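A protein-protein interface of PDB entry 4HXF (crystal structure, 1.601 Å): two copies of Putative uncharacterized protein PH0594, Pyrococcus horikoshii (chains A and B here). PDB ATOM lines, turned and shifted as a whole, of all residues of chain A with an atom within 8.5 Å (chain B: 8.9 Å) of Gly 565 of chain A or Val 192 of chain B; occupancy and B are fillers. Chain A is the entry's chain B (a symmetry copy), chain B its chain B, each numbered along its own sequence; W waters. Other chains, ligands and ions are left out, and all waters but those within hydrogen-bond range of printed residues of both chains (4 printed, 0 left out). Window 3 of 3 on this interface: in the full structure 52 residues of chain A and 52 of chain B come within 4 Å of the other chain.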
ATOM      1  N   ALA A 531      11.054  35.729   6.793  1.00  0.00           N
ATOM      2  CA  ALA A 531      11.853  34.470   6.847  1.00  0.00           C
ATOM      3  C   ALA A 531      12.922  34.356   5.774  1.00  0.00           C
ATOM      4  O   ALA A 531      13.964  33.788   6.059  1.00  0.00           O
ATOM      5  CB  ALA A 531      10.852  33.321   6.751  1.00  0.00           C
ATOM      6  N   LYS A 532      12.665  34.845   4.567  1.00  0.00           N
ATOM      7  CA  LYS A 532      13.669  34.745   3.490  1.00  0.00           C
ATOM      8  C   LYS A 532      15.018  35.391   3.847  1.00  0.00           C
ATOM      9  O   LYS A 532      16.032  35.053   3.305  1.00  0.00           O
ATOM     10  CB  LYS A 532      13.101  35.219   2.142  1.00  0.00           C
ATOM     11  CG  LYS A 532      12.891  36.700   2.119  1.00  0.00           C
ATOM     12  CD  LYS A 532      12.373  37.270   0.775  1.00  0.00           C
ATOM     13  CE  LYS A 532      11.650  38.630   1.037  1.00  0.00           C
ATOM     14  N   VAL A 534      16.666  35.264   6.667  1.00  0.00           N
ATOM     15  CA  VAL A 534      17.468  34.553   7.696  1.00  0.00           C
ATOM     16  C   VAL A 534      18.698  33.900   7.067  1.00  0.00           C
ATOM     17  O   VAL A 534      18.597  33.224   5.986  1.00  0.00           O
ATOM     18  CB  VAL A 534      16.665  33.536   8.466  1.00  0.00           C
ATOM     19  CG1 VAL A 534      17.530  32.702   9.462  1.00  0.00           C
ATOM     20  CG2 VAL A 534      15.486  34.211   9.152  1.00  0.00           C
ATOM     21  N   TYR A 558       9.412  27.462  11.778  1.00  0.00           N
ATOM     22  CA  TYR A 558      10.188  26.300  11.400  1.00  0.00           C
ATOM     23  C   TYR A 558       9.839  25.777   9.995  1.00  0.00           C
ATOM     24  O   TYR A 558      10.739  25.681   9.103  1.00  0.00           O
ATOM     25  CB  TYR A 558      10.007  25.175  12.416  1.00  0.00           C
ATOM     26  CG  TYR A 558      10.763  23.901  12.011  1.00  0.00           C
ATOM     27  CD1 TYR A 558      12.137  23.806  12.131  1.00  0.00           C
ATOM     28  CD2 TYR A 558      10.105  22.878  11.395  1.00  0.00           C
ATOM     29  CE1 TYR A 558      12.821  22.680  11.685  1.00  0.00           C
ATOM     30  CE2 TYR A 558      10.757  21.768  10.905  1.00  0.00           C
ATOM     31  CZ  TYR A 558      12.139  21.675  11.074  1.00  0.00           C
ATOM     32  OH  TYR A 558      12.863  20.603  10.603  1.00  0.00           O
ATOM     33  N   HIS A 559       8.540  25.495   9.735  1.00  0.00           N
ATOM     34  CA  HIS A 559       8.184  24.993   8.407  1.00  0.00           C
ATOM     35  C   HIS A 559       8.509  25.937   7.244  1.00  0.00           C
ATOM     36  O   HIS A 559       8.963  25.533   6.168  1.00  0.00           O
ATOM     37  CB  HIS A 559       6.685  24.641   8.322  1.00  0.00           C
ATOM     38  CG  HIS A 559       6.275  23.417   9.056  1.00  0.00           C
ATOM     39  ND1 HIS A 559       4.980  23.163   9.429  1.00  0.00           N
ATOM     40  CD2 HIS A 559       6.997  22.208   9.334  1.00  0.00           C
ATOM     41  CE1 HIS A 559       4.919  21.852   9.948  1.00  0.00           C
ATOM     42  NE2 HIS A 559       6.138  21.306   9.859  1.00  0.00           N
ATOM     43  N   VAL A 560       8.214  27.229   7.495  1.00  0.00           N
ATOM     44  CA  VAL A 560       8.420  28.246   6.465  1.00  0.00           C
ATOM     45  C   VAL A 560       9.893  28.411   6.224  1.00  0.00           C
ATOM     46  O   VAL A 560      10.326  28.495   5.051  1.00  0.00           O
ATOM     47  CB  VAL A 560       7.695  29.552   6.792  1.00  0.00           C
ATOM     48  CG1 VAL A 560       8.258  30.674   5.942  1.00  0.00           C
ATOM     49  CG2 VAL A 560       6.156  29.390   6.671  1.00  0.00           C
ATOM     50  N   LEU A 561      10.699  28.474   7.265  1.00  0.00           N
ATOM     51  CA  LEU A 561      12.186  28.524   7.079  1.00  0.00           C
ATOM     52  C   LEU A 561      12.721  27.276   6.324  1.00  0.00           C
ATOM     53  O   LEU A 561      13.525  27.416   5.395  1.00  0.00           O
ATOM     54  CB  LEU A 561      12.903  28.733   8.476  1.00  0.00           C
ATOM     55  CG  LEU A 561      12.743  30.090   9.111  1.00  0.00           C
ATOM     56  CD1 LEU A 561      13.123  29.934  10.567  1.00  0.00           C
ATOM     57  CD2 LEU A 561      13.564  31.130   8.345  1.00  0.00           C
ATOM     58  N   LYS A 562      12.193  26.092   6.589  1.00  0.00           N
ATOM     59  CA  LYS A 562      12.589  24.933   5.858  1.00  0.00           C
ATOM     60  C   LYS A 562      12.122  25.034   4.377  1.00  0.00           C
ATOM     61  O   LYS A 562      12.862  24.628   3.472  1.00  0.00           O
ATOM     62  CB  LYS A 562      11.980  23.669   6.497  1.00  0.00           C
ATOM     63  CG  LYS A 562      12.653  23.295   7.828  1.00  0.00           C
ATOM     64  CD  LYS A 562      14.104  22.837   7.774  1.00  0.00           C
ATOM     65  CE  LYS A 562      14.278  21.716   6.932  1.00  0.00           C
ATOM     66  NZ  LYS A 562      15.768  21.217   6.910  1.00  0.00           N
ATOM     67  N   ASP A 563      10.936  25.610   4.147  1.00  0.00           N
ATOM     68  CA  ASP A 563      10.374  25.750   2.780  1.00  0.00           C
ATOM     69  C   ASP A 563      11.292  26.671   1.949  1.00  0.00           C
ATOM     70  O   ASP A 563      11.328  26.603   0.735  1.00  0.00           O
ATOM     71  CB  ASP A 563       8.998  26.359   2.836  1.00  0.00           C
ATOM     72  CG  ASP A 563       8.118  26.022   1.650  1.00  0.00           C
ATOM     73  OD1 ASP A 563       8.353  25.023   0.964  1.00  0.00           O
ATOM     74  OD2 ASP A 563       7.167  26.796   1.410  1.00  0.00           O
ATOM     75  N   LEU A 564      12.063  27.514   2.697  1.00  0.00           N
ATOM     76  CA  LEU A 564      12.976  28.511   2.102  1.00  0.00           C
ATOM     77  C   LEU A 564      14.421  28.008   2.136  1.00  0.00           C
ATOM     78  O   LEU A 564      15.363  28.758   1.786  1.00  0.00           O
ATOM     79  CB  LEU A 564      12.776  29.874   2.744  1.00  0.00           C
ATOM     80  CG  LEU A 564      11.433  30.514   2.510  1.00  0.00           C
ATOM     81  CD1 LEU A 564      11.216  31.736   3.452  1.00  0.00           C
ATOM     82  CD2 LEU A 564      11.216  30.925   1.050  1.00  0.00           C
ATOM     83  N   GLY A 565      14.633  26.732   2.463  1.00  0.00           N
ATOM     84  CA  GLY A 565      15.995  26.159   2.408  1.00  0.00           C
ATOM     85  C   GLY A 565      16.924  26.594   3.540  1.00  0.00           C
ATOM     86  O   GLY A 565      18.132  26.370   3.434  1.00  0.00           O
ATOM     87  N   LYS A 566      16.411  27.058   4.663  1.00  0.00           N
ATOM     88  CA  LYS A 566      17.274  27.534   5.777  1.00  0.00           C
ATOM     89  C   LYS A 566      17.657  26.382   6.696  1.00  0.00           C
ATOM     90  O   LYS A 566      16.959  25.391   6.770  1.00  0.00           O
ATOM     91  CB  LYS A 566      16.505  28.567   6.562  1.00  0.00           C
ATOM     92  CG  LYS A 566      15.887  29.717   5.728  1.00  0.00           C
ATOM     93  CD  LYS A 566      16.888  30.526   4.943  1.00  0.00           C
ATOM     94  CE  LYS A 566      16.249  31.738   4.313  1.00  0.00           C
ATOM     95  NZ  LYS A 566      17.283  32.566   3.628  1.00  0.00           N
ATOM     96  N   GLU A 567      18.754  26.569   7.375  1.00  0.00           N
ATOM     97  CA  GLU A 567      19.199  25.663   8.400  1.00  0.00           C
ATOM     98  C   GLU A 567      18.477  26.019   9.692  1.00  0.00           C
ATOM     99  O   GLU A 567      18.808  27.004  10.365  1.00  0.00           O
ATOM    100  CB  GLU A 567      20.736  25.802   8.596  1.00  0.00           C
ATOM    101  CG  GLU A 567      21.180  24.807   9.665  1.00  0.00           C
ATOM    102  CD  GLU A 567      22.687  24.791  10.007  1.00  0.00           C
ATOM    103  OE1 GLU A 567      23.028  24.010  10.892  1.00  0.00           O
ATOM    104  OE2 GLU A 567      23.511  25.502   9.381  1.00  0.00           O
ATOM    105  N   VAL A 568      17.554  25.177  10.096  1.00  0.00           N
ATOM    106  CA  VAL A 568      16.685  25.388  11.249  1.00  0.00           C
ATOM    107  C   VAL A 568      16.336  24.034  11.848  1.00  0.00           C
ATOM    108  O   VAL A 568      16.316  23.027  11.089  1.00  0.00           O
ATOM    109  CB  VAL A 568      15.463  26.238  10.900  1.00  0.00           C
ATOM    110  CG1 VAL A 568      14.600  25.525   9.862  1.00  0.00           C
ATOM    111  CG2 VAL A 568      14.730  26.691  12.229  1.00  0.00           C
ATOM    112  N   ASP B 135      14.368  18.031  12.082  1.00  0.00           N
ATOM    113  CA  ASP B 135      15.246  18.775  11.192  1.00  0.00           C
ATOM    114  C   ASP B 135      14.866  18.557   9.706  1.00  0.00           C
ATOM    115  O   ASP B 135      15.578  19.069   8.815  1.00  0.00           O
ATOM    116  CB  ASP B 135      16.729  18.369  11.378  1.00  0.00           C
ATOM    117  CG  ASP B 135      17.013  16.938  10.900  1.00  0.00           C
ATOM    118  OD1 ASP B 135      16.122  16.238  10.433  1.00  0.00           O
ATOM    119  OD2 ASP B 135      18.182  16.514  11.004  1.00  0.00           O
ATOM    120  N   ASP B 136      13.721  17.926   9.482  1.00  0.00           N
ATOM    121  CA  ASP B 136      13.127  17.753   8.117  1.00  0.00           C
ATOM    122  C   ASP B 136      11.709  18.372   8.096  1.00  0.00           C
ATOM    123  O   ASP B 136      11.355  19.137   9.041  1.00  0.00           O
ATOM    124  CB  ASP B 136      13.203  16.302   7.697  1.00  0.00           C
ATOM    125  CG  ASP B 136      13.051  16.147   6.164  1.00  0.00           C
ATOM    126  OD1 ASP B 136      12.877  17.090   5.420  1.00  0.00           O
ATOM    127  OD2 ASP B 136      13.315  15.055   5.817  1.00  0.00           O
ATOM    128  N   VAL B 137      10.864  18.069   7.074  1.00  0.00           N
ATOM    129  CA  VAL B 137       9.525  18.645   7.039  1.00  0.00           C
ATOM    130  C   VAL B 137       8.637  17.543   6.537  1.00  0.00           C
ATOM    131  O   VAL B 137       9.094  16.662   5.819  1.00  0.00           O
ATOM    132  CB  VAL B 137       9.317  19.916   6.135  1.00  0.00           C
ATOM    133  CG1 VAL B 137      10.006  21.103   6.712  1.00  0.00           C
ATOM    134  CG2 VAL B 137       9.706  19.621   4.689  1.00  0.00           C
ATOM    135  N   HIS B 189      10.812  12.265  -3.729  1.00  0.00           N
ATOM    136  CA  HIS B 189      11.939  12.944  -4.273  1.00  0.00           C
ATOM    137  C   HIS B 189      12.244  14.187  -3.459  1.00  0.00           C
ATOM    138  O   HIS B 189      11.326  14.879  -3.136  1.00  0.00           O
ATOM    139  CB  HIS B 189      11.642  13.337  -5.753  1.00  0.00           C
ATOM    140  CG  HIS B 189      12.771  14.060  -6.389  1.00  0.00           C
ATOM    141  ND1 HIS B 189      13.800  13.445  -7.017  1.00  0.00           N
ATOM    142  CD2 HIS B 189      13.029  15.443  -6.471  1.00  0.00           C
ATOM    143  CE1 HIS B 189      14.671  14.399  -7.437  1.00  0.00           C
ATOM    144  NE2 HIS B 189      14.194  15.599  -7.070  1.00  0.00           N
ATOM    145  N   ARG B 190      13.519  14.455  -3.258  1.00  0.00           N
ATOM    146  CA  ARG B 190      13.883  15.628  -2.440  1.00  0.00           C
ATOM    147  C   ARG B 190      14.408  16.785  -3.291  1.00  0.00           C
ATOM    148  O   ARG B 190      15.439  16.629  -3.971  1.00  0.00           O
ATOM    149  CB  ARG B 190      14.887  15.290  -1.356  1.00  0.00           C
ATOM    150  CG  ARG B 190      15.074  16.476  -0.378  1.00  0.00           C
ATOM    151  CD  ARG B 190      16.132  16.132   0.729  1.00  0.00           C
ATOM    152  NE  ARG B 190      15.705  15.041   1.630  1.00  0.00           N
ATOM    153  CZ  ARG B 190      14.939  15.251   2.713  1.00  0.00           C
ATOM    154  NH1 ARG B 190      14.558  16.439   2.997  1.00  0.00           N
ATOM    155  NH2 ARG B 190      14.518  14.227   3.421  1.00  0.00           N
ATOM    156  N   ASP B 191      13.749  17.934  -3.242  1.00  0.00           N
ATOM    157  CA  ASP B 191      14.305  19.215  -3.777  1.00  0.00           C
ATOM    158  C   ASP B 191      14.644  20.117  -2.575  1.00  0.00           C
ATOM    159  O   ASP B 191      15.472  19.696  -1.786  1.00  0.00           O
ATOM    160  CB  ASP B 191      13.343  19.872  -4.723  1.00  0.00           C
ATOM    161  CG  ASP B 191      13.149  18.990  -6.058  1.00  0.00           C
ATOM    162  OD1 ASP B 191      14.100  18.521  -6.563  1.00  0.00           O
ATOM    163  OD2 ASP B 191      12.069  18.951  -6.484  1.00  0.00           O
ATOM    164  N   VAL B 192      14.012  21.277  -2.391  1.00  0.00           N
ATOM    165  CA  VAL B 192      14.340  22.116  -1.139  1.00  0.00           C
ATOM    166  C   VAL B 192      13.720  21.360   0.077  1.00  0.00           C
ATOM    167  O   VAL B 192      14.364  21.236   1.087  1.00  0.00           O
ATOM    168  CB  VAL B 192      13.778  23.487  -1.289  1.00  0.00           C
ATOM    169  CG1 VAL B 192      13.915  24.290   0.020  1.00  0.00           C
ATOM    170  CG2 VAL B 192      14.558  24.230  -2.408  1.00  0.00           C
ATOM    171  N   ILE B 193      12.563  20.741  -0.164  1.00  0.00           N
ATOM    172  CA  ILE B 193      11.909  19.856   0.728  1.00  0.00           C
ATOM    173  C   ILE B 193      11.520  18.603  -0.022  1.00  0.00           C
ATOM    174  O   ILE B 193      11.534  18.558  -1.271  1.00  0.00           O
ATOM    175  CB  ILE B 193      10.695  20.500   1.386  1.00  0.00           C
ATOM    176  CG1 ILE B 193       9.575  20.889   0.439  1.00  0.00           C
ATOM    177  CG2 ILE B 193      11.201  21.808   2.125  1.00  0.00           C
ATOM    178  CD1 ILE B 193       8.198  21.246   1.116  1.00  0.00           C
ATOM    179  N   PRO B 194      11.106  17.548   0.684  1.00  0.00           N
ATOM    180  CA  PRO B 194      10.538  16.388  -0.040  1.00  0.00           C
ATOM    181  C   PRO B 194       9.263  16.737  -0.777  1.00  0.00           C
ATOM    182  O   PRO B 194       8.419  17.461  -0.267  1.00  0.00           O
ATOM    183  CB  PRO B 194      10.294  15.326   1.071  1.00  0.00           C
ATOM    184  CG  PRO B 194      11.112  15.799   2.214  1.00  0.00           C
ATOM    185  CD  PRO B 194      11.129  17.317   2.130  1.00  0.00           C
ATOM    186  N   ARG B 195       9.139  16.216  -1.989  1.00  0.00           N
ATOM    187  CA  ARG B 195       7.985  16.510  -2.863  1.00  0.00           C
ATOM    188  C   ARG B 195       6.826  15.529  -2.679  1.00  0.00           C
ATOM    189  O   ARG B 195       6.382  14.762  -3.589  1.00  0.00           O
ATOM    190  CB  ARG B 195       8.470  16.596  -4.295  1.00  0.00           C
ATOM    191  CG  ARG B 195       9.655  17.440  -4.540  1.00  0.00           C
ATOM    192  CD  ARG B 195       9.412  18.928  -4.240  1.00  0.00           C
ATOM    193  NE  ARG B 195       8.289  19.567  -4.919  1.00  0.00           N
ATOM    194  CZ  ARG B 195       8.394  20.102  -6.143  1.00  0.00           C
ATOM    195  NH1 ARG B 195       9.511  19.992  -6.835  1.00  0.00           N
ATOM    196  NH2 ARG B 195       7.338  20.705  -6.662  1.00  0.00           N
ATOM    197  N   LYS B 216      12.331  11.390 -10.194  1.00  0.00           N
ATOM    198  CA  LYS B 216      11.413  12.543 -10.147  1.00  0.00           C
ATOM    199  C   LYS B 216      10.213  12.338 -11.065  1.00  0.00           C
ATOM    200  O   LYS B 216       9.953  13.149 -12.019  1.00  0.00           O
ATOM    201  CB  LYS B 216      12.158  13.846 -10.412  1.00  0.00           C
ATOM    202  CG  LYS B 216      11.397  15.061 -10.001  1.00  0.00           C
ATOM    203  CD  LYS B 216      12.340  16.329 -10.046  1.00  0.00           C
ATOM    204  CE  LYS B 216      11.663  17.550  -9.546  1.00  0.00           C
ATOM    205  NZ  LYS B 216      12.798  18.501  -9.153  1.00  0.00           N
ATOM    206  N   LEU B 505       2.629  22.999   3.185  1.00  0.00           N
ATOM    207  CA  LEU B 505       3.738  23.677   2.510  1.00  0.00           C
ATOM    208  C   LEU B 505       3.604  23.504   0.975  1.00  0.00           C
ATOM    209  O   LEU B 505       4.000  24.439   0.242  1.00  0.00           O
ATOM    210  CB  LEU B 505       5.113  23.209   2.986  1.00  0.00           C
ATOM    211  CG  LEU B 505       5.609  23.642   4.346  1.00  0.00           C
ATOM    212  CD1 LEU B 505       6.989  22.994   4.593  1.00  0.00           C
ATOM    213  CD2 LEU B 505       5.554  25.185   4.424  1.00  0.00           C
ATOM    214  N   LYS B 509      -0.090  25.824  -1.515  1.00  0.00           N
ATOM    215  CA  LYS B 509       0.511  26.534  -2.713  1.00  0.00           C
ATOM    216  C   LYS B 509      -0.335  26.266  -3.968  1.00  0.00           C
ATOM    217  O   LYS B 509      -0.492  27.173  -4.826  1.00  0.00           O
ATOM    218  CB  LYS B 509       1.986  26.245  -2.942  1.00  0.00           C
ATOM    219  CG  LYS B 509       2.875  26.939  -1.887  1.00  0.00           C
ATOM    220  CD  LYS B 509       4.340  26.804  -2.220  1.00  0.00           C
ATOM    221  CE  LYS B 509       5.246  27.387  -1.125  1.00  0.00           C
ATOM    222  NZ  LYS B 509       6.680  27.049  -1.328  1.00  0.00           N
HETATM  223  O   HOH W   1      15.889  18.869   5.389  1.00  0.00           O
HETATM  224  O   HOH W   2       6.636  24.143  -0.740  1.00  0.00           O
HETATM  225  O   HOH W   3       9.053  28.650  -0.379  1.00  0.00           O
HETATM  226  O   HOH W   4      14.835  22.853   3.466  1.00  0.00           O
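The side-chain amino group of Lys 509 of chain B lies within salt-bridge range of the side-chain carboxylate of Asp 563 of chain A. The backbone carbonyl oxygen (O) of Asp 136 of chain B is in hydrogen-bond range of the side-chain hydroxyl (OH) of Tyr 558 of chain A (2.6 Å). The backbone NH (N) of Asp 135 of chain B sits close to the side-chain hydroxyl (OH) of Tyr 558 of chain A, at 3.3 Å. The backbone carbonyl oxygen of Asp 135 of chain B sits at hydrogen-bond distance from the side-chain amino group of Lys 562 of chain A (2.9 Å).
The guanidinium group of Arg 190 of chain B lies within salt-bridge range of the side-chain carboxylate of Asp 136 of chain B.
Leu 505 of chain B touches His 559 of chain A (CD1 to O, 3.6 Å). Val 137 of chain B touches Lys 562 of chain A (CG1 to CB, 3.2 Å). O of Lys 562 of chain A touches CG1 of Val 192 of chain B, 3.6 Å away. O of Lys 562 of chain A touches CG2 of Ile 193 of chain B (3.5 Å). Val 192 of chain B touches Asp 563 of chain A (CG1 to O, 3.5 Å). Asp 563 of chain A touches Ile 193 of chain B (OD1 to CD1, 3.8 Å). Asp 563 of chain A touches Leu 505 of chain B (OD2 to CD2, 3.8 Å). Gly 565 of chain A touches Val 192 of chain B (N to CG1, 3.5 Å).
Printed residues of chain B within 4 Å of Gly 565 of chain A: Val 192 (3.5 Å). Of the printed residues of chain A, Val 192 of chain B touches Lys 562, Asp 563 and Gly 565. Printed residues of chain A within 4 Å of Asp 136 of chain B: Tyr 558. Of the printed residues of chain B, Tyr 558 of chain A touches Asp 135 and Asp 136. Printed residues of chain B within 4 Å of Lys 562 of chain A: Asp 135 (2.9 Å), Val 137 (3.2 Å), Val 192 (3.6 Å) and Ile 193 (3.5 Å). Leu 564 of chain A touches none of the printed residues of chain B. The nearest printed residue of chain B that does not touch His 559 of chain A is Val 137 of chain B (4.1 Å).
Hydrophobic or aromatic side chains of chain B that line the printed part of chain A: Val 137, Val 192, Ile 193 and Leu 505. Of the 14 printed residues of chain A, 5 touch a printed residue of chain B. Hydrophobic or aromatic side chains of chain A that line the printed part of chain B: Tyr 558. Along chain A the printed residues that touch a printed residue of chain B span positions 558 to 565. Among the printed residues, 12 pairs touch across the chains. Among the printed residues, Asp or Glu carboxylates within 4 Å of a Lys or Arg side-chain nitrogen of the other chain: Asp 563 of chain A with Lys 509 of chain B (2.8 Å).
No position is printed for both chains.
Water W2 lies within hydrogen-bond range of OD1 of Asp 563 of chain A (2.6 Å), O of Leu 505 of chain B (2.8 Å) and NZ of Lys 509 of chain B (3.0 Å). Water W4 lies within hydrogen-bond range of O of Lys 562 of chain A and O of Val 192 of chain B. Water W1 lies within hydrogen-bond range of NZ of Lys 562 of chain A, O of Asp 135 of chain B and OD1 of Asp 136 of chain B. Water W3 bridges the side-chain amino group (NZ) of Lys 509 of chain B (3.0 Å) and the side-chain carboxylate (OD2) of Asp 563 of chain A (3.2 Å).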
